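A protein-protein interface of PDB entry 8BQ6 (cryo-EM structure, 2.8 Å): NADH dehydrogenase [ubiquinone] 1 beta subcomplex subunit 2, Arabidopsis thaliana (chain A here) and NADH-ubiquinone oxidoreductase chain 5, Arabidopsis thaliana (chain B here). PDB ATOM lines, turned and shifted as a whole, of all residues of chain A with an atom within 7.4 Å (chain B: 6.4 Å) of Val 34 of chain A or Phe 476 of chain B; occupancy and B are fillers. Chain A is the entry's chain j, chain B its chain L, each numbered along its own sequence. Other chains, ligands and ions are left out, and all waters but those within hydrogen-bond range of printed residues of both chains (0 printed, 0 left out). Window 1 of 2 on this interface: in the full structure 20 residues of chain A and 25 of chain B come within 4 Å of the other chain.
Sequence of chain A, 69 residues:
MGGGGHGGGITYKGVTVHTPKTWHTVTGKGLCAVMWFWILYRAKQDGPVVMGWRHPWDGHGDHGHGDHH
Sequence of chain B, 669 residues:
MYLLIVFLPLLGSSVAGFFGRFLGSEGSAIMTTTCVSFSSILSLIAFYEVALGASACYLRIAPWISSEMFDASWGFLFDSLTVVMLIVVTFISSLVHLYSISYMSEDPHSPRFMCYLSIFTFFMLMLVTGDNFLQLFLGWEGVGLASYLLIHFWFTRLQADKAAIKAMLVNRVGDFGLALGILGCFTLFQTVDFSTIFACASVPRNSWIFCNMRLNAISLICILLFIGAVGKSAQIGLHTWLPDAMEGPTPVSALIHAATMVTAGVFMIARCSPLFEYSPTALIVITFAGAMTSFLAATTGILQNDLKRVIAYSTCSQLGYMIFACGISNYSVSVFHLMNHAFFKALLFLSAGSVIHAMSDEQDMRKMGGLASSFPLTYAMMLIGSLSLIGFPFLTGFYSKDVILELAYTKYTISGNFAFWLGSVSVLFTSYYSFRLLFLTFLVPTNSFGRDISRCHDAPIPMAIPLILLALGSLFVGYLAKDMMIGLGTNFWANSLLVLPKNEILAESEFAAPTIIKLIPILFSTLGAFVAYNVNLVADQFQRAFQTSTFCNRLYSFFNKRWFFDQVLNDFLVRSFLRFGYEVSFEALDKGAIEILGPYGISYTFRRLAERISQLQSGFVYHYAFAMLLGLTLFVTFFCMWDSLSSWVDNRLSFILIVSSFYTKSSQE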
ATOM      1  N   GLY A  28     -12.177  18.614 -17.053  1.00  0.00           N
ATOM      2  CA  GLY A  28     -11.854  18.040 -15.737  1.00  0.00           C
ATOM      3  C   GLY A  28     -10.358  17.944 -15.532  1.00  0.00           C
ATOM      4  O   GLY A  28      -9.871  18.489 -14.522  1.00  0.00           O
ATOM      5  N   LYS A  29      -9.655  17.289 -16.466  1.00  0.00           N
ATOM      6  CA  LYS A  29      -8.205  17.164 -16.356  1.00  0.00           C
ATOM      7  C   LYS A  29      -7.538  18.533 -16.357  1.00  0.00           C
ATOM      8  O   LYS A  29      -6.585  18.778 -15.610  1.00  0.00           O
ATOM      9  CB  LYS A  29      -7.657  16.319 -17.506  1.00  0.00           C
ATOM     10  CG  LYS A  29      -8.173  14.898 -17.567  1.00  0.00           C
ATOM     11  CD  LYS A  29      -8.079  14.378 -18.991  1.00  0.00           C
ATOM     12  CE  LYS A  29      -6.674  13.901 -19.327  1.00  0.00           C
ATOM     13  NZ  LYS A  29      -5.941  13.448 -18.118  1.00  0.00           N
ATOM     14  N   GLY A  30      -8.019  19.431 -17.218  1.00  0.00           N
ATOM     15  CA  GLY A  30      -7.387  20.732 -17.345  1.00  0.00           C
ATOM     16  C   GLY A  30      -7.529  21.587 -16.103  1.00  0.00           C
ATOM     17  O   GLY A  30      -6.564  22.217 -15.661  1.00  0.00           O
ATOM     18  N   LEU A  31      -8.730  21.599 -15.527  1.00  0.00           N
ATOM     19  CA  LEU A  31      -8.992  22.473 -14.351  1.00  0.00           C
ATOM     20  C   LEU A  31      -8.154  21.996 -13.163  1.00  0.00           C
ATOM     21  O   LEU A  31      -7.556  22.852 -12.493  1.00  0.00           O
ATOM     22  CB  LEU A  31     -10.486  22.443 -14.016  1.00  0.00           C
ATOM     23  CG  LEU A  31     -10.946  23.436 -12.952  1.00  0.00           C
ATOM     24  CD1 LEU A  31     -12.361  23.923 -13.227  1.00  0.00           C
ATOM     25  CD2 LEU A  31     -10.852  22.827 -11.563  1.00  0.00           C
ATOM     26  N   CYS A  32      -8.122  20.688 -12.915  1.00  0.00           N
ATOM     27  CA  CYS A  32      -7.275  20.164 -11.814  1.00  0.00           C
ATOM     28  C   CYS A  32      -5.791  20.392 -12.133  1.00  0.00           C
ATOM     29  O   CYS A  32      -5.078  20.743 -11.212  1.00  0.00           O
ATOM     30  CB  CYS A  32      -7.559  18.694 -11.547  1.00  0.00           C
ATOM     31  SG  CYS A  32      -8.854  18.427 -10.309  1.00  0.00           S
ATOM     32  N   ALA A  33      -5.344  20.225 -13.383  1.00  0.00           N
ATOM     33  CA  ALA A  33      -3.955  20.523 -13.719  1.00  0.00           C
ATOM     34  C   ALA A  33      -3.630  21.985 -13.448  1.00  0.00           C
ATOM     35  O   ALA A  33      -2.560  22.302 -12.914  1.00  0.00           O
ATOM     36  CB  ALA A  33      -3.673  20.176 -15.181  1.00  0.00           C
ATOM     37  N   VAL A  34      -4.549  22.884 -13.802  1.00  0.00           N
ATOM     38  CA  VAL A  34      -4.403  24.295 -13.456  1.00  0.00           C
ATOM     39  C   VAL A  34      -4.285  24.452 -11.945  1.00  0.00           C
ATOM     40  O   VAL A  34      -3.539  25.303 -11.444  1.00  0.00           O
ATOM     41  CB  VAL A  34      -5.596  25.089 -14.025  1.00  0.00           C
ATOM     42  CG1 VAL A  34      -5.794  26.409 -13.289  1.00  0.00           C
ATOM     43  CG2 VAL A  34      -5.437  25.300 -15.523  1.00  0.00           C
ATOM     44  N   MET A  35      -5.010  23.613 -11.201  1.00  0.00           N
ATOM     45  CA  MET A  35      -4.981  23.657  -9.743  1.00  0.00           C
ATOM     46  C   MET A  35      -3.657  23.146  -9.190  1.00  0.00           C
ATOM     47  O   MET A  35      -3.083  23.743  -8.271  1.00  0.00           O
ATOM     48  CB  MET A  35      -6.143  22.832  -9.193  1.00  0.00           C
ATOM     49  CG  MET A  35      -6.086  22.596  -7.710  1.00  0.00           C
ATOM     50  SD  MET A  35      -7.057  21.168  -7.221  1.00  0.00           S
ATOM     51  CE  MET A  35      -7.395  21.616  -5.531  1.00  0.00           C
ATOM     52  N   TRP A  36      -3.169  22.020  -9.716  1.00  0.00           N
ATOM     53  CA  TRP A  36      -1.900  21.472  -9.243  1.00  0.00           C
ATOM     54  C   TRP A  36      -0.754  22.435  -9.507  1.00  0.00           C
ATOM     55  O   TRP A  36       0.110  22.636  -8.647  1.00  0.00           O
ATOM     56  CB  TRP A  36      -1.626  20.127  -9.910  1.00  0.00           C
ATOM     57  CG  TRP A  36      -2.651  19.104  -9.594  1.00  0.00           C
ATOM     58  CD1 TRP A  36      -3.448  18.442 -10.477  1.00  0.00           C
ATOM     59  CD2 TRP A  36      -2.992  18.612  -8.296  1.00  0.00           C
ATOM     60  NE1 TRP A  36      -4.273  17.573  -9.809  1.00  0.00           N
ATOM     61  CE2 TRP A  36      -4.010  17.655  -8.468  1.00  0.00           C
ATOM     62  CE3 TRP A  36      -2.535  18.888  -7.005  1.00  0.00           C
ATOM     63  CZ2 TRP A  36      -4.580  16.977  -7.399  1.00  0.00           C
ATOM     64  CZ3 TRP A  36      -3.103  18.214  -5.946  1.00  0.00           C
ATOM     65  CH2 TRP A  36      -4.113  17.269  -6.149  1.00  0.00           C
ATOM     66  N   PHE A  37      -0.731  23.036 -10.696  1.00  0.00           N
ATOM     67  CA  PHE A  37       0.309  24.004 -11.020  1.00  0.00           C
ATOM     68  C   PHE A  37       0.255  25.212 -10.094  1.00  0.00           C
ATOM     69  O   PHE A  37       1.286  25.637  -9.561  1.00  0.00           O
ATOM     70  CB  PHE A  37       0.171  24.438 -12.477  1.00  0.00           C
ATOM     71  CG  PHE A  37       1.126  25.517 -12.874  1.00  0.00           C
ATOM     72  CD1 PHE A  37       2.411  25.205 -13.274  1.00  0.00           C
ATOM     73  CD2 PHE A  37       0.735  26.845 -12.858  1.00  0.00           C
ATOM     74  CE1 PHE A  37       3.292  26.197 -13.640  1.00  0.00           C
ATOM     75  CE2 PHE A  37       1.608  27.839 -13.222  1.00  0.00           C
ATOM     76  CZ  PHE A  37       2.889  27.518 -13.613  1.00  0.00           C
ATOM     77  N   TRP A  38      -0.940  25.769  -9.886  1.00  0.00           N
ATOM     78  CA  TRP A  38      -1.078  26.940  -9.026  1.00  0.00           C
ATOM     79  C   TRP A  38      -0.606  26.643  -7.610  1.00  0.00           C
ATOM     80  O   TRP A  38      -0.121  27.536  -6.903  1.00  0.00           O
ATOM     81  CB  TRP A  38      -2.533  27.406  -9.024  1.00  0.00           C
ATOM     82  CG  TRP A  38      -2.891  28.278  -7.871  1.00  0.00           C
ATOM     83  CD1 TRP A  38      -3.562  27.910  -6.743  1.00  0.00           C
ATOM     84  CD2 TRP A  38      -2.600  29.671  -7.729  1.00  0.00           C
ATOM     85  NE1 TRP A  38      -3.707  28.988  -5.906  1.00  0.00           N
ATOM     86  CE2 TRP A  38      -3.125  30.082  -6.489  1.00  0.00           C
ATOM     87  CE3 TRP A  38      -1.945  30.611  -8.528  1.00  0.00           C
ATOM     88  CZ2 TRP A  38      -3.017  31.391  -6.032  1.00  0.00           C
ATOM     89  CZ3 TRP A  38      -1.839  31.910  -8.073  1.00  0.00           C
ATOM     90  CH2 TRP A  38      -2.372  32.288  -6.837  1.00  0.00           C
ATOM     91  N   ILE A  39      -0.748  25.391  -7.177  1.00  0.00           N
ATOM     92  CA  ILE A  39      -0.281  24.999  -5.852  1.00  0.00           C
ATOM     93  C   ILE A  39       1.240  24.939  -5.818  1.00  0.00           C
ATOM     94  O   ILE A  39       1.874  25.445  -4.884  1.00  0.00           O
ATOM     95  CB  ILE A  39      -0.902  23.650  -5.459  1.00  0.00           C
ATOM     96  CG1 ILE A  39      -2.379  23.835  -5.133  1.00  0.00           C
ATOM     97  CG2 ILE A  39      -0.178  23.068  -4.264  1.00  0.00           C
ATOM     98  CD1 ILE A  39      -3.080  22.551  -4.831  1.00  0.00           C
ATOM     99  N   LEU A  40       1.847  24.303  -6.824  1.00  0.00           N
ATOM    100  CA  LEU A  40       3.304  24.252  -6.886  1.00  0.00           C
ATOM    101  C   LEU A  40       3.886  25.647  -7.046  1.00  0.00           C
ATOM    102  O   LEU A  40       4.897  25.985  -6.420  1.00  0.00           O
ATOM    103  CB  LEU A  40       3.755  23.348  -8.033  1.00  0.00           C
ATOM    104  CG  LEU A  40       3.387  21.868  -7.907  1.00  0.00           C
ATOM    105  CD1 LEU A  40       3.759  21.093  -9.166  1.00  0.00           C
ATOM    106  CD2 LEU A  40       4.061  21.272  -6.689  1.00  0.00           C
ATOM    107  N   PHE B 394      -2.877  27.140   0.055  1.00  0.00           N
ATOM    108  CA  PHE B 394      -2.981  28.070  -1.068  1.00  0.00           C
ATOM    109  C   PHE B 394      -4.279  27.946  -1.850  1.00  0.00           C
ATOM    110  O   PHE B 394      -4.362  28.482  -2.960  1.00  0.00           O
ATOM    111  CB  PHE B 394      -1.799  27.937  -2.036  1.00  0.00           C
ATOM    112  CG  PHE B 394      -0.494  27.772  -1.341  1.00  0.00           C
ATOM    113  CD1 PHE B 394      -0.020  28.770  -0.509  1.00  0.00           C
ATOM    114  CD2 PHE B 394       0.237  26.609  -1.475  1.00  0.00           C
ATOM    115  CE1 PHE B 394       1.169  28.623   0.156  1.00  0.00           C
ATOM    116  CE2 PHE B 394       1.430  26.455  -0.811  1.00  0.00           C
ATOM    117  CZ  PHE B 394       1.898  27.465   0.007  1.00  0.00           C
ATOM    118  N   LEU B 395      -5.289  27.261  -1.327  1.00  0.00           N
ATOM    119  CA  LEU B 395      -6.606  27.349  -1.933  1.00  0.00           C
ATOM    120  C   LEU B 395      -7.439  28.403  -1.214  1.00  0.00           C
ATOM    121  O   LEU B 395      -6.982  29.064  -0.280  1.00  0.00           O
ATOM    122  CB  LEU B 395      -7.312  25.996  -1.910  1.00  0.00           C
ATOM    123  CG  LEU B 395      -6.519  24.825  -2.477  1.00  0.00           C
ATOM    124  CD1 LEU B 395      -7.405  23.606  -2.558  1.00  0.00           C
ATOM    125  CD2 LEU B 395      -5.985  25.197  -3.849  1.00  0.00           C
ATOM    126  N   THR B 396      -8.684  28.557  -1.664  1.00  0.00           N
ATOM    127  CA  THR B 396      -9.537  29.600  -1.104  1.00  0.00           C
ATOM    128  C   THR B 396      -9.799  29.377   0.379  1.00  0.00           C
ATOM    129  O   THR B 396      -9.788  30.329   1.166  1.00  0.00           O
ATOM    130  CB  THR B 396     -10.852  29.678  -1.873  1.00  0.00           C
ATOM    131  OG1 THR B 396     -10.578  29.771  -3.277  1.00  0.00           O
ATOM    132  CG2 THR B 396     -11.647  30.891  -1.431  1.00  0.00           C
ATOM    133  N   ALA B 471     -15.441  26.481  -9.463  1.00  0.00           N
ATOM    134  CA  ALA B 471     -14.097  25.871  -9.302  1.00  0.00           C
ATOM    135  C   ALA B 471     -13.068  26.994  -9.332  1.00  0.00           C
ATOM    136  O   ALA B 471     -12.278  27.073  -8.387  1.00  0.00           O
ATOM    137  CB  ALA B 471     -13.828  24.860 -10.379  1.00  0.00           C
ATOM    138  N   LEU B 472     -13.131  27.857 -10.351  1.00  0.00           N
ATOM    139  CA  LEU B 472     -12.209  29.027 -10.423  1.00  0.00           C
ATOM    140  C   LEU B 472     -12.308  29.845  -9.130  1.00  0.00           C
ATOM    141  O   LEU B 472     -11.250  30.227  -8.606  1.00  0.00           O
ATOM    142  CB  LEU B 472     -12.554  29.875 -11.647  1.00  0.00           C
ATOM    143  CG  LEU B 472     -12.320  29.195 -12.994  1.00  0.00           C
ATOM    144  CD1 LEU B 472     -12.806  30.073 -14.133  1.00  0.00           C
ATOM    145  CD2 LEU B 472     -10.852  28.846 -13.175  1.00  0.00           C
ATOM    146  N   GLY B 473     -13.522  30.090  -8.624  1.00  0.00           N
ATOM    147  CA  GLY B 473     -13.667  30.791  -7.331  1.00  0.00           C
ATOM    148  C   GLY B 473     -13.020  30.016  -6.191  1.00  0.00           C
ATOM    149  O   GLY B 473     -12.195  30.612  -5.482  1.00  0.00           O
ATOM    150  N   SER B 474     -13.336  28.724  -6.043  1.00  0.00           N
ATOM    151  CA  SER B 474     -12.802  27.869  -4.944  1.00  0.00           C
ATOM    152  C   SER B 474     -11.310  27.555  -5.110  1.00  0.00           C
ATOM    153  O   SER B 474     -10.834  26.652  -4.402  1.00  0.00           O
ATOM    154  CB  SER B 474     -13.573  26.586  -4.856  1.00  0.00           C
ATOM    155  OG  SER B 474     -14.967  26.821  -4.945  1.00  0.00           O
ATOM    156  N   LEU B 475     -10.596  28.268  -5.986  1.00  0.00           N
ATOM    157  CA  LEU B 475      -9.141  28.063  -6.184  1.00  0.00           C
ATOM    158  C   LEU B 475      -8.424  29.400  -6.069  1.00  0.00           C
ATOM    159  O   LEU B 475      -7.316  29.416  -5.512  1.00  0.00           O
ATOM    160  CB  LEU B 475      -8.911  27.508  -7.594  1.00  0.00           C
ATOM    161  CG  LEU B 475      -9.156  26.018  -7.782  1.00  0.00           C
ATOM    162  CD1 LEU B 475      -8.784  25.586  -9.191  1.00  0.00           C
ATOM    163  CD2 LEU B 475      -8.389  25.221  -6.745  1.00  0.00           C
ATOM    164  N   PHE B 476      -9.050  30.482  -6.531  1.00  0.00           N
ATOM    165  CA  PHE B 476      -8.316  31.773  -6.614  1.00  0.00           C
ATOM    166  C   PHE B 476      -8.933  32.897  -5.773  1.00  0.00           C
ATOM    167  O   PHE B 476      -8.207  33.872  -5.523  1.00  0.00           O
ATOM    168  CB  PHE B 476      -8.241  32.182  -8.088  1.00  0.00           C
ATOM    169  CG  PHE B 476      -7.620  31.143  -8.989  1.00  0.00           C
ATOM    170  CD1 PHE B 476      -6.345  30.657  -8.740  1.00  0.00           C
ATOM    171  CD2 PHE B 476      -8.312  30.639 -10.078  1.00  0.00           C
ATOM    172  CE1 PHE B 476      -5.781  29.691  -9.558  1.00  0.00           C
ATOM    173  CE2 PHE B 476      -7.745  29.675 -10.897  1.00  0.00           C
ATOM    174  CZ  PHE B 476      -6.479  29.204 -10.636  1.00  0.00           C
ATOM    175  N   VAL B 477     -10.200  32.797  -5.370  1.00  0.00           N
ATOM    176  CA  VAL B 477     -10.837  33.951  -4.664  1.00  0.00           C
ATOM    177  C   VAL B 477     -10.076  34.235  -3.366  1.00  0.00           C
ATOM    178  O   VAL B 477      -9.813  35.418  -3.091  1.00  0.00           O
ATOM    179  CB  VAL B 477     -12.348  33.722  -4.437  1.00  0.00           C
ATOM    180  CG1 VAL B 477     -12.865  34.309  -3.133  1.00  0.00           C
ATOM    181  CG2 VAL B 477     -13.164  34.243  -5.607  1.00  0.00           C
ATOM    182  N   GLY B 478      -9.658  33.194  -2.649  1.00  0.00           N
ATOM    183  CA  GLY B 478      -9.047  33.399  -1.351  1.00  0.00           C
ATOM    184  C   GLY B 478      -7.752  34.178  -1.414  1.00  0.00           C
ATOM    185  O   GLY B 478      -7.560  35.129  -0.652  1.00  0.00           O
ATOM    186  N   TYR B 479      -6.860  33.794  -2.331  1.00  0.00           N
ATOM    187  CA  TYR B 479      -5.602  34.515  -2.492  1.00  0.00           C
ATOM    188  C   TYR B 479      -5.845  35.946  -2.957  1.00  0.00           C
ATOM    189  O   TYR B 479      -5.218  36.889  -2.466  1.00  0.00           O
ATOM    190  CB  TYR B 479      -4.698  33.777  -3.481  1.00  0.00           C
ATOM    191  CG  TYR B 479      -3.525  34.592  -3.978  1.00  0.00           C
ATOM    192  CD1 TYR B 479      -2.388  34.757  -3.200  1.00  0.00           C
ATOM    193  CD2 TYR B 479      -3.560  35.204  -5.224  1.00  0.00           C
ATOM    194  CE1 TYR B 479      -1.319  35.500  -3.653  1.00  0.00           C
ATOM    195  CE2 TYR B 479      -2.498  35.949  -5.682  1.00  0.00           C
ATOM    196  CZ  TYR B 479      -1.380  36.096  -4.894  1.00  0.00           C
ATOM    197  OH  TYR B 479      -0.317  36.839  -5.348  1.00  0.00           O
ATOM    198  N   LEU B 480      -6.767  36.121  -3.909  1.00  0.00           N
ATOM    199  CA  LEU B 480      -6.983  37.431  -4.514  1.00  0.00           C
ATOM    200  C   LEU B 480      -7.573  38.435  -3.532  1.00  0.00           C
ATOM    201  O   LEU B 480      -7.336  39.640  -3.664  1.00  0.00           O
ATOM    202  CB  LEU B 480      -7.902  37.301  -5.727  1.00  0.00           C
ATOM    203  CG  LEU B 480      -7.296  37.421  -7.126  1.00  0.00           C
ATOM    204  CD1 LEU B 480      -6.759  38.820  -7.347  1.00  0.00           C
ATOM    205  CD2 LEU B 480      -6.210  36.390  -7.353  1.00  0.00           C
ATOM    206  N   ALA B 481      -8.355  37.971  -2.560  1.00  0.00           N
ATOM    207  CA  ALA B 481      -9.120  38.863  -1.702  1.00  0.00           C
ATOM    208  C   ALA B 481      -8.571  38.976  -0.287  1.00  0.00           C
ATOM    209  O   ALA B 481      -9.187  39.653   0.541  1.00  0.00           O
ATOM    210  CB  ALA B 481     -10.585  38.411  -1.651  1.00  0.00           C
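The backbone carbonyl oxygen of Phe 394 of chain B sits at hydrogen-bond distance from the indole nitrogen of Trp 38 of chain A, at 3.1 Å.
OG1 of Thr 396 of chain B is in hydrogen-bond range of N of Leu 475 of chain B (3.1 Å).
Among the printed residues, merely in contact across the chains: Leu 31 of chain A with Ala 471 of chain B, Trp 38 of chain A with Tyr 479 of chain B, Met 35 of chain A with Leu 395 of chain B, Met 35 of chain A with Leu 475 of chain B, Trp 38 of chain A with Phe 476 of chain B, Trp 38 of chain A with Leu 475 of chain B, Val 34 of chain A with Phe 476 of chain B and Ile 39 of chain A with Phe 394 of chain B.
Printed residues of chain B within 4 Å of Leu 31 of chain A: Ala 471. Of chain B, only Phe 476 comes within 4 Å of Val 34 of chain A. Printed residues of chain A within 4 Å of Ala 471 of chain B: Leu 31. The nearest residue of chain B that does not touch Val 34 of chain A is Leu 475 of chain B (5.1 Å). The nearest residue of chain A that does not touch Phe 476 of chain B is Met 35 of chain A (5.8 Å).
Of the 13 printed residues of chain A, 5 touch a printed residue of chain B. Hydrophobic or aromatic side chains of chain A that line the printed part of chain B: Leu 31, Val 34, Met 35 and Trp 38. Among the printed residues, no Asp or Glu carboxylate lies within 4 Å of a Lys or Arg side-chain nitrogen of the other chain.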
